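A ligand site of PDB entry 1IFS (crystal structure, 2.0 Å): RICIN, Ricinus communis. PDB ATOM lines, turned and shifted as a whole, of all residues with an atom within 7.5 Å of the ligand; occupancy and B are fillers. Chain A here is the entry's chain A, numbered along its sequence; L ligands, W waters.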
ATOM      1  N   ALA A  73     -20.981 -29.188   0.081  1.00  0.00           N
ATOM      2  CA  ALA A  73     -20.783 -30.285   1.014  1.00  0.00           C
ATOM      3  C   ALA A  73     -19.767 -29.838   2.049  1.00  0.00           C
ATOM      4  O   ALA A  73     -18.705 -29.346   1.694  1.00  0.00           O
ATOM      5  CB  ALA A  73     -20.278 -31.525   0.284  1.00  0.00           C
ATOM      6  N   LEU A  74     -20.127 -29.937   3.321  1.00  0.00           N
ATOM      7  CA  LEU A  74     -19.213 -29.564   4.398  1.00  0.00           C
ATOM      8  C   LEU A  74     -18.772 -30.826   5.125  1.00  0.00           C
ATOM      9  O   LEU A  74     -19.560 -31.755   5.311  1.00  0.00           O
ATOM     10  CB  LEU A  74     -19.877 -28.601   5.389  1.00  0.00           C
ATOM     11  CG  LEU A  74     -20.073 -27.105   5.082  1.00  0.00           C
ATOM     12  CD1 LEU A  74     -21.028 -26.881   3.928  1.00  0.00           C
ATOM     13  CD2 LEU A  74     -20.632 -26.447   6.325  1.00  0.00           C
ATOM     14  N   ASP A  75     -17.509 -30.884   5.481  1.00  0.00           N
ATOM     15  CA  ASP A  75     -16.972 -32.026   6.195  1.00  0.00           C
ATOM     16  C   ASP A  75     -17.244 -31.693   7.658  1.00  0.00           C
ATOM     17  O   ASP A  75     -16.877 -30.623   8.160  1.00  0.00           O
ATOM     18  CB  ASP A  75     -15.474 -32.123   5.910  1.00  0.00           C
ATOM     19  CG  ASP A  75     -14.803 -33.268   6.618  1.00  0.00           C
ATOM     20  OD1 ASP A  75     -15.297 -33.711   7.678  1.00  0.00           O
ATOM     21  OD2 ASP A  75     -13.750 -33.703   6.137  1.00  0.00           O
ATOM     22  N   ASN A  78     -14.272 -30.571  10.480  1.00  0.00           N
ATOM     23  CA  ASN A  78     -13.602 -29.267  10.432  1.00  0.00           C
ATOM     24  C   ASN A  78     -14.431 -28.138   9.831  1.00  0.00           C
ATOM     25  O   ASN A  78     -13.963 -27.009   9.738  1.00  0.00           O
ATOM     26  CB  ASN A  78     -12.280 -29.361   9.667  1.00  0.00           C
ATOM     27  CG  ASN A  78     -12.453 -29.915   8.255  1.00  0.00           C
ATOM     28  OD1 ASN A  78     -13.564 -29.992   7.723  1.00  0.00           O
ATOM     29  ND2 ASN A  78     -11.349 -30.325   7.655  1.00  0.00           N
ATOM     30  N   ALA A  79     -15.665 -28.437   9.426  1.00  0.00           N
ATOM     31  CA  ALA A  79     -16.589 -27.465   8.810  1.00  0.00           C
ATOM     32  C   ALA A  79     -16.095 -26.925   7.472  1.00  0.00           C
ATOM     33  O   ALA A  79     -16.540 -25.880   7.010  1.00  0.00           O
ATOM     34  CB  ALA A  79     -16.890 -26.331   9.775  1.00  0.00           C
ATOM     35  N   TYR A  80     -15.224 -27.676   6.818  1.00  0.00           N
ATOM     36  CA  TYR A  80     -14.674 -27.282   5.532  1.00  0.00           C
ATOM     37  C   TYR A  80     -15.628 -27.592   4.387  1.00  0.00           C
ATOM     38  O   TYR A  80     -16.300 -28.626   4.416  1.00  0.00           O
ATOM     39  CB  TYR A  80     -13.389 -28.073   5.278  1.00  0.00           C
ATOM     40  CG  TYR A  80     -12.110 -27.319   5.534  1.00  0.00           C
ATOM     41  CD1 TYR A  80     -11.786 -26.850   6.800  1.00  0.00           C
ATOM     42  CD2 TYR A  80     -11.206 -27.079   4.486  1.00  0.00           C
ATOM     43  CE1 TYR A  80     -10.605 -26.153   7.039  1.00  0.00           C
ATOM     44  CE2 TYR A  80     -10.026 -26.381   4.715  1.00  0.00           C
ATOM     45  CZ  TYR A  80      -9.736 -25.919   5.982  1.00  0.00           C
ATOM     46  OH  TYR A  80      -8.593 -25.183   6.200  1.00  0.00           O
ATOM     47  N   VAL A  81     -15.660 -26.716   3.384  1.00  0.00           N
ATOM     48  CA  VAL A  81     -16.471 -26.947   2.176  1.00  0.00           C
ATOM     49  C   VAL A  81     -15.562 -27.857   1.307  1.00  0.00           C
ATOM     50  O   VAL A  81     -14.456 -27.451   0.954  1.00  0.00           O
ATOM     51  CB  VAL A  81     -16.717 -25.641   1.388  1.00  0.00           C
ATOM     52  CG1 VAL A  81     -17.472 -25.942   0.103  1.00  0.00           C
ATOM     53  CG2 VAL A  81     -17.514 -24.682   2.241  1.00  0.00           C
ATOM     54  N   VAL A  82     -16.002 -29.070   1.015  1.00  0.00           N
ATOM     55  CA  VAL A  82     -15.196 -30.005   0.227  1.00  0.00           C
ATOM     56  C   VAL A  82     -15.501 -29.998  -1.266  1.00  0.00           C
ATOM     57  O   VAL A  82     -14.689 -30.429  -2.090  1.00  0.00           O
ATOM     58  CB  VAL A  82     -15.302 -31.465   0.769  1.00  0.00           C
ATOM     59  CG1 VAL A  82     -14.927 -31.507   2.230  1.00  0.00           C
ATOM     60  CG2 VAL A  82     -16.704 -32.026   0.587  1.00  0.00           C
ATOM     61  N   GLY A  83     -16.697 -29.531  -1.608  1.00  0.00           N
ATOM     62  CA  GLY A  83     -17.104 -29.497  -2.988  1.00  0.00           C
ATOM     63  C   GLY A  83     -18.537 -29.043  -3.098  1.00  0.00           C
ATOM     64  O   GLY A  83     -19.174 -28.755  -2.074  1.00  0.00           O
ATOM     65  N   PHE A  93     -12.697 -30.238  -4.392  1.00  0.00           N
ATOM     66  CA  PHE A  93     -11.348 -29.700  -4.283  1.00  0.00           C
ATOM     67  C   PHE A  93     -10.420 -30.931  -4.227  1.00  0.00           C
ATOM     68  O   PHE A  93     -10.863 -32.037  -3.876  1.00  0.00           O
ATOM     69  CB  PHE A  93     -11.160 -28.876  -3.004  1.00  0.00           C
ATOM     70  CG  PHE A  93     -11.849 -27.558  -3.035  1.00  0.00           C
ATOM     71  CD1 PHE A  93     -11.513 -26.598  -3.989  1.00  0.00           C
ATOM     72  CD2 PHE A  93     -12.815 -27.236  -2.071  1.00  0.00           C
ATOM     73  CE1 PHE A  93     -12.120 -25.338  -3.974  1.00  0.00           C
ATOM     74  CE2 PHE A  93     -13.422 -25.976  -2.056  1.00  0.00           C
ATOM     75  CZ  PHE A  93     -13.072 -25.015  -3.010  1.00  0.00           C
ATOM     76  N   GLY A 120      -6.492 -27.423  -4.175  1.00  0.00           N
ATOM     77  CA  GLY A 120      -7.234 -27.609  -2.941  1.00  0.00           C
ATOM     78  C   GLY A 120      -8.025 -26.361  -2.583  1.00  0.00           C
ATOM     79  O   GLY A 120      -7.883 -25.325  -3.238  1.00  0.00           O
ATOM     80  N   GLY A 121      -8.769 -26.415  -1.477  1.00  0.00           N
ATOM     81  CA  GLY A 121      -9.589 -25.298  -1.072  1.00  0.00           C
ATOM     82  C   GLY A 121      -9.080 -24.365   0.009  1.00  0.00           C
ATOM     83  O   GLY A 121      -9.854 -23.626   0.585  1.00  0.00           O
ATOM     84  N   ASN A 122      -7.791 -24.400   0.318  1.00  0.00           N
ATOM     85  CA  ASN A 122      -7.263 -23.489   1.332  1.00  0.00           C
ATOM     86  C   ASN A 122      -7.234 -22.051   0.780  1.00  0.00           C
ATOM     87  O   ASN A 122      -7.171 -21.854  -0.429  1.00  0.00           O
ATOM     88  CB  ASN A 122      -5.859 -23.921   1.773  1.00  0.00           C
ATOM     89  CG  ASN A 122      -4.887 -23.957   0.629  1.00  0.00           C
ATOM     90  OD1 ASN A 122      -4.100 -23.039   0.430  1.00  0.00           O
ATOM     91  ND2 ASN A 122      -4.941 -25.025  -0.153  1.00  0.00           N
ATOM     92  N   TYR A 123      -7.253 -21.052   1.654  1.00  0.00           N
ATOM     93  CA  TYR A 123      -7.268 -19.682   1.193  1.00  0.00           C
ATOM     94  C   TYR A 123      -6.084 -19.279   0.336  1.00  0.00           C
ATOM     95  O   TYR A 123      -6.265 -18.583  -0.644  1.00  0.00           O
ATOM     96  CB  TYR A 123      -7.407 -18.705   2.354  1.00  0.00           C
ATOM     97  CG  TYR A 123      -8.750 -18.748   3.043  1.00  0.00           C
ATOM     98  CD1 TYR A 123      -9.953 -18.585   2.337  1.00  0.00           C
ATOM     99  CD2 TYR A 123      -8.806 -18.933   4.416  1.00  0.00           C
ATOM    100  CE1 TYR A 123     -11.191 -18.604   3.025  1.00  0.00           C
ATOM    101  CE2 TYR A 123      -9.995 -18.942   5.094  1.00  0.00           C
ATOM    102  CZ  TYR A 123     -11.182 -18.784   4.417  1.00  0.00           C
ATOM    103  OH  TYR A 123     -12.318 -18.774   5.187  1.00  0.00           O
ATOM    104  N   ASP A 124      -4.888 -19.731   0.671  1.00  0.00           N
ATOM    105  CA  ASP A 124      -3.730 -19.340  -0.126  1.00  0.00           C
ATOM    106  C   ASP A 124      -3.898 -19.652  -1.594  1.00  0.00           C
ATOM    107  O   ASP A 124      -3.732 -18.780  -2.444  1.00  0.00           O
ATOM    108  CB  ASP A 124      -2.471 -20.019   0.387  1.00  0.00           C
ATOM    109  CG  ASP A 124      -1.841 -19.254   1.532  1.00  0.00           C
ATOM    110  OD1 ASP A 124      -1.731 -18.016   1.437  1.00  0.00           O
ATOM    111  OD2 ASP A 124      -1.454 -19.901   2.542  1.00  0.00           O
ATOM    112  N   LEU A 126      -6.708 -20.416  -3.224  1.00  0.00           N
ATOM    113  CA  LEU A 126      -7.874 -19.717  -3.718  1.00  0.00           C
ATOM    114  C   LEU A 126      -7.630 -18.231  -4.006  1.00  0.00           C
ATOM    115  O   LEU A 126      -8.155 -17.693  -4.989  1.00  0.00           O
ATOM    116  CB  LEU A 126      -9.038 -19.904  -2.749  1.00  0.00           C
ATOM    117  CG  LEU A 126     -10.125 -20.953  -3.019  1.00  0.00           C
ATOM    118  CD1 LEU A 126      -9.684 -22.115  -3.864  1.00  0.00           C
ATOM    119  CD2 LEU A 126     -10.671 -21.414  -1.685  1.00  0.00           C
ATOM    120  N   ARG A 134      -8.266 -11.947   0.709  1.00  0.00           N
ATOM    121  CA  ARG A 134      -9.495 -11.848   1.501  1.00  0.00           C
ATOM    122  C   ARG A 134      -9.822 -10.410   1.893  1.00  0.00           C
ATOM    123  O   ARG A 134     -10.958  -9.950   1.781  1.00  0.00           O
ATOM    124  CB  ARG A 134      -9.374 -12.722   2.765  1.00  0.00           C
ATOM    125  CG  ARG A 134      -9.748 -14.160   2.529  1.00  0.00           C
ATOM    126  CD  ARG A 134      -9.439 -15.027   3.735  1.00  0.00           C
ATOM    127  NE  ARG A 134      -7.991 -15.244   3.848  1.00  0.00           N
ATOM    128  CZ  ARG A 134      -7.367 -15.578   4.977  1.00  0.00           C
ATOM    129  NH1 ARG A 134      -8.035 -15.750   6.108  1.00  0.00           N
ATOM    130  NH2 ARG A 134      -6.066 -15.772   4.959  1.00  0.00           N
ATOM    131  N   PHE A 168     -15.890 -18.935  -4.058  1.00  0.00           N
ATOM    132  CA  PHE A 168     -15.655 -19.904  -3.001  1.00  0.00           C
ATOM    133  C   PHE A 168     -15.211 -19.156  -1.748  1.00  0.00           C
ATOM    134  O   PHE A 168     -15.665 -19.461  -0.653  1.00  0.00           O
ATOM    135  CB  PHE A 168     -14.555 -20.897  -3.417  1.00  0.00           C
ATOM    136  CG  PHE A 168     -15.066 -22.068  -4.197  1.00  0.00           C
ATOM    137  CD1 PHE A 168     -16.143 -22.829  -3.719  1.00  0.00           C
ATOM    138  CD2 PHE A 168     -14.440 -22.464  -5.372  1.00  0.00           C
ATOM    139  CE1 PHE A 168     -16.589 -23.962  -4.423  1.00  0.00           C
ATOM    140  CE2 PHE A 168     -14.879 -23.591  -6.076  1.00  0.00           C
ATOM    141  CZ  PHE A 168     -15.949 -24.344  -5.597  1.00  0.00           C
ATOM    142  N   ILE A 172     -17.161 -19.673   1.651  1.00  0.00           N
ATOM    143  CA  ILE A 172     -16.486 -20.255   2.802  1.00  0.00           C
ATOM    144  C   ILE A 172     -16.521 -19.349   4.047  1.00  0.00           C
ATOM    145  O   ILE A 172     -16.758 -19.826   5.159  1.00  0.00           O
ATOM    146  CB  ILE A 172     -15.033 -20.672   2.418  1.00  0.00           C
ATOM    147  CG1 ILE A 172     -15.061 -21.782   1.372  1.00  0.00           C
ATOM    148  CG2 ILE A 172     -14.240 -21.084   3.636  1.00  0.00           C
ATOM    149  CD1 ILE A 172     -13.748 -21.975   0.670  1.00  0.00           C
ATOM    150  N   GLN A 173     -16.345 -18.039   3.880  1.00  0.00           N
ATOM    151  CA  GLN A 173     -16.384 -17.143   5.022  1.00  0.00           C
ATOM    152  C   GLN A 173     -17.784 -16.897   5.554  1.00  0.00           C
ATOM    153  O   GLN A 173     -17.963 -16.742   6.754  1.00  0.00           O
ATOM    154  CB  GLN A 173     -15.726 -15.804   4.715  1.00  0.00           C
ATOM    155  CG  GLN A 173     -14.230 -15.902   4.553  1.00  0.00           C
ATOM    156  CD  GLN A 173     -13.634 -14.605   4.079  1.00  0.00           C
ATOM    157  OE1 GLN A 173     -13.687 -14.298   2.887  1.00  0.00           O
ATOM    158  NE2 GLN A 173     -13.100 -13.825   4.987  1.00  0.00           N
ATOM    159  N   SER A 176     -18.885 -21.471   6.498  1.00  0.00           N
ATOM    160  CA  SER A 176     -17.985 -22.167   7.402  1.00  0.00           C
ATOM    161  C   SER A 176     -17.366 -21.302   8.515  1.00  0.00           C
ATOM    162  O   SER A 176     -17.375 -21.713   9.680  1.00  0.00           O
ATOM    163  CB  SER A 176     -16.881 -22.859   6.615  1.00  0.00           C
ATOM    164  OG  SER A 176     -17.469 -23.753   5.698  1.00  0.00           O
ATOM    165  N   GLU A 177     -16.825 -20.137   8.161  1.00  0.00           N
ATOM    166  CA  GLU A 177     -16.217 -19.291   9.180  1.00  0.00           C
ATOM    167  C   GLU A 177     -17.240 -18.704  10.146  1.00  0.00           C
ATOM    168  O   GLU A 177     -16.946 -18.542  11.325  1.00  0.00           O
ATOM    169  CB  GLU A 177     -15.361 -18.184   8.565  1.00  0.00           C
ATOM    170  CG  GLU A 177     -14.269 -18.702   7.619  1.00  0.00           C
ATOM    171  CD  GLU A 177     -13.109 -19.365   8.302  1.00  0.00           C
ATOM    172  OE1 GLU A 177     -13.219 -19.683   9.501  1.00  0.00           O
ATOM    173  OE2 GLU A 177     -12.077 -19.557   7.645  1.00  0.00           O
ATOM    174  N   ARG A 180     -18.053 -21.273  12.651  1.00  0.00           N
ATOM    175  CA  ARG A 180     -16.966 -21.469  13.591  1.00  0.00           C
ATOM    176  C   ARG A 180     -16.844 -20.396  14.656  1.00  0.00           C
ATOM    177  O   ARG A 180     -16.489 -20.708  15.792  1.00  0.00           O
ATOM    178  CB  ARG A 180     -15.637 -21.518  12.855  1.00  0.00           C
ATOM    179  CG  ARG A 180     -15.419 -22.745  12.029  1.00  0.00           C
ATOM    180  CD  ARG A 180     -14.247 -22.504  11.111  1.00  0.00           C
ATOM    181  NE  ARG A 180     -13.834 -23.715  10.412  1.00  0.00           N
ATOM    182  CZ  ARG A 180     -13.175 -23.712   9.260  1.00  0.00           C
ATOM    183  NH1 ARG A 180     -12.878 -22.570   8.668  1.00  0.00           N
ATOM    184  NH2 ARG A 180     -12.843 -24.849   8.690  1.00  0.00           N
ATOM    185  N   GLU A 208      -9.756 -16.243  11.396  1.00  0.00           N
ATOM    186  CA  GLU A 208      -9.826 -17.306  10.402  1.00  0.00           C
ATOM    187  C   GLU A 208      -8.519 -18.051  10.360  1.00  0.00           C
ATOM    188  O   GLU A 208      -8.493 -19.278  10.339  1.00  0.00           O
ATOM    189  CB  GLU A 208     -10.141 -16.758   9.013  1.00  0.00           C
ATOM    190  CG  GLU A 208     -11.507 -16.147   8.921  1.00  0.00           C
ATOM    191  CD  GLU A 208     -11.788 -15.488   7.592  1.00  0.00           C
ATOM    192  OE1 GLU A 208     -10.873 -15.305   6.768  1.00  0.00           O
ATOM    193  OE2 GLU A 208     -12.947 -15.105   7.395  1.00  0.00           O
ATOM    194  N   TRP A 211      -7.881 -20.347  13.835  1.00  0.00           N
ATOM    195  CA  TRP A 211      -8.816 -21.348  14.342  1.00  0.00           C
ATOM    196  C   TRP A 211      -8.157 -22.633  14.839  1.00  0.00           C
ATOM    197  O   TRP A 211      -8.473 -23.100  15.927  1.00  0.00           O
ATOM    198  CB  TRP A 211      -9.872 -21.657  13.294  1.00  0.00           C
ATOM    199  CG  TRP A 211     -10.967 -22.554  13.767  1.00  0.00           C
ATOM    200  CD1 TRP A 211     -11.904 -22.270  14.712  1.00  0.00           C
ATOM    201  CD2 TRP A 211     -11.308 -23.842  13.242  1.00  0.00           C
ATOM    202  NE1 TRP A 211     -12.821 -23.286  14.807  1.00  0.00           N
ATOM    203  CE2 TRP A 211     -12.486 -24.267  13.911  1.00  0.00           C
ATOM    204  CE3 TRP A 211     -10.754 -24.671  12.252  1.00  0.00           C
ATOM    205  CZ2 TRP A 211     -13.115 -25.492  13.626  1.00  0.00           C
ATOM    206  CZ3 TRP A 211     -11.377 -25.889  11.968  1.00  0.00           C
ATOM    207  CH2 TRP A 211     -12.548 -26.281  12.653  1.00  0.00           C
HETATM  208  N1  LIG L   1     -10.690 -22.499   5.101  1.00  0.00           N
HETATM  209  C1  LIG L   1     -10.042 -22.437   3.899  1.00  0.00           C
HETATM  210  N2  LIG L   1     -10.602 -23.117   2.961  1.00  0.00           N
HETATM  211  C2  LIG L   1     -11.693 -23.686   3.567  1.00  0.00           C
HETATM  212  C3  LIG L   1     -12.661 -24.526   3.076  1.00  0.00           C
HETATM  213  N3  LIG L   1     -12.661 -24.946   1.814  1.00  0.00           N
HETATM  214  N4  LIG L   1     -13.590 -24.888   3.969  1.00  0.00           N
HETATM  215  C4  LIG L   1     -13.521 -24.432   5.205  1.00  0.00           C
HETATM  216  N5  LIG L   1     -12.667 -23.649   5.792  1.00  0.00           N
HETATM  217  C5  LIG L   1     -11.760 -23.319   4.874  1.00  0.00           C
HETATM  218  O   HOH W   1      -6.901 -22.373   4.371  1.00  0.00           O
HETATM  219  O   HOH W   2      -9.801 -20.970   7.653  1.00  0.00           O
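O of Ile 172 lies within hydrogen-bond range of N of Glu 177. O of Tyr 80 is in hydrogen-bond range of N of Asp 75. O of Ala 79 lies within hydrogen-bond range of OG of Ser 176. The side-chain amide oxygen of Asn 78 is in hydrogen-bond range of the backbone NH of Tyr 80. OE2 of Glu 177 is in hydrogen-bond range of OH of Tyr 123 (2.6 Å). The side-chain amide oxygen of Asn 122 sits close to the backbone NH of Asp 124, 3.4 Å away. NH1 of Arg 180 is in salt-bridge range of OE1 of Glu 177 (3.0 Å). The guanidinium group (NH2) of Arg 180 lies within hydrogen-bond range of the backbone carbonyl oxygen (O) of Asn 78 (2.6 Å).
Ala 79 touches the ligand. CA of Tyr 80 touches N4 of the ligand, at 3.1 Å. Asn 122 touches the ligand (CA to N2, 3.7 Å). CE2 of Tyr 123 touches N1 of the ligand (3.6 Å). Ile 172 touches the ligand (CD1 to N3, 3.4 Å). Ser 176 touches the ligand. Hydrophobic or aromatic side chains within 4 Å of the ligand: Tyr 80, Tyr 123 and Ile 172. Nine residues have an atom within 4 Å of the ligand: Ala 79, Tyr 80, Val 81, Gly 121, Asn 122, Tyr 123, Ile 172, Ser 176 and Arg 180. Along chain A the residues within 4 Å of the ligand span positions 79 to 180. The nearest printed residue that does not touch the ligand is Phe 93 (4.1 Å).
Water W2 lies within hydrogen-bond range of OE2 of Glu 177, N1 of the ligand and O of Glu 208.
The backbone NH (N) of Val 81 is in hydrogen-bond range of a nitrogen (N4) of the ligand (2.8 Å). The backbone carbonyl oxygen (O) of Val 81 sits at hydrogen-bond distance from a nitrogen (N3) of the ligand (3.2 Å). N3 of the ligand sits at hydrogen-bond distance from O of Gly 121, 3.3 Å away. N5 of the ligand is in hydrogen-bond range of NH1 of Arg 180 (3.1 Å).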
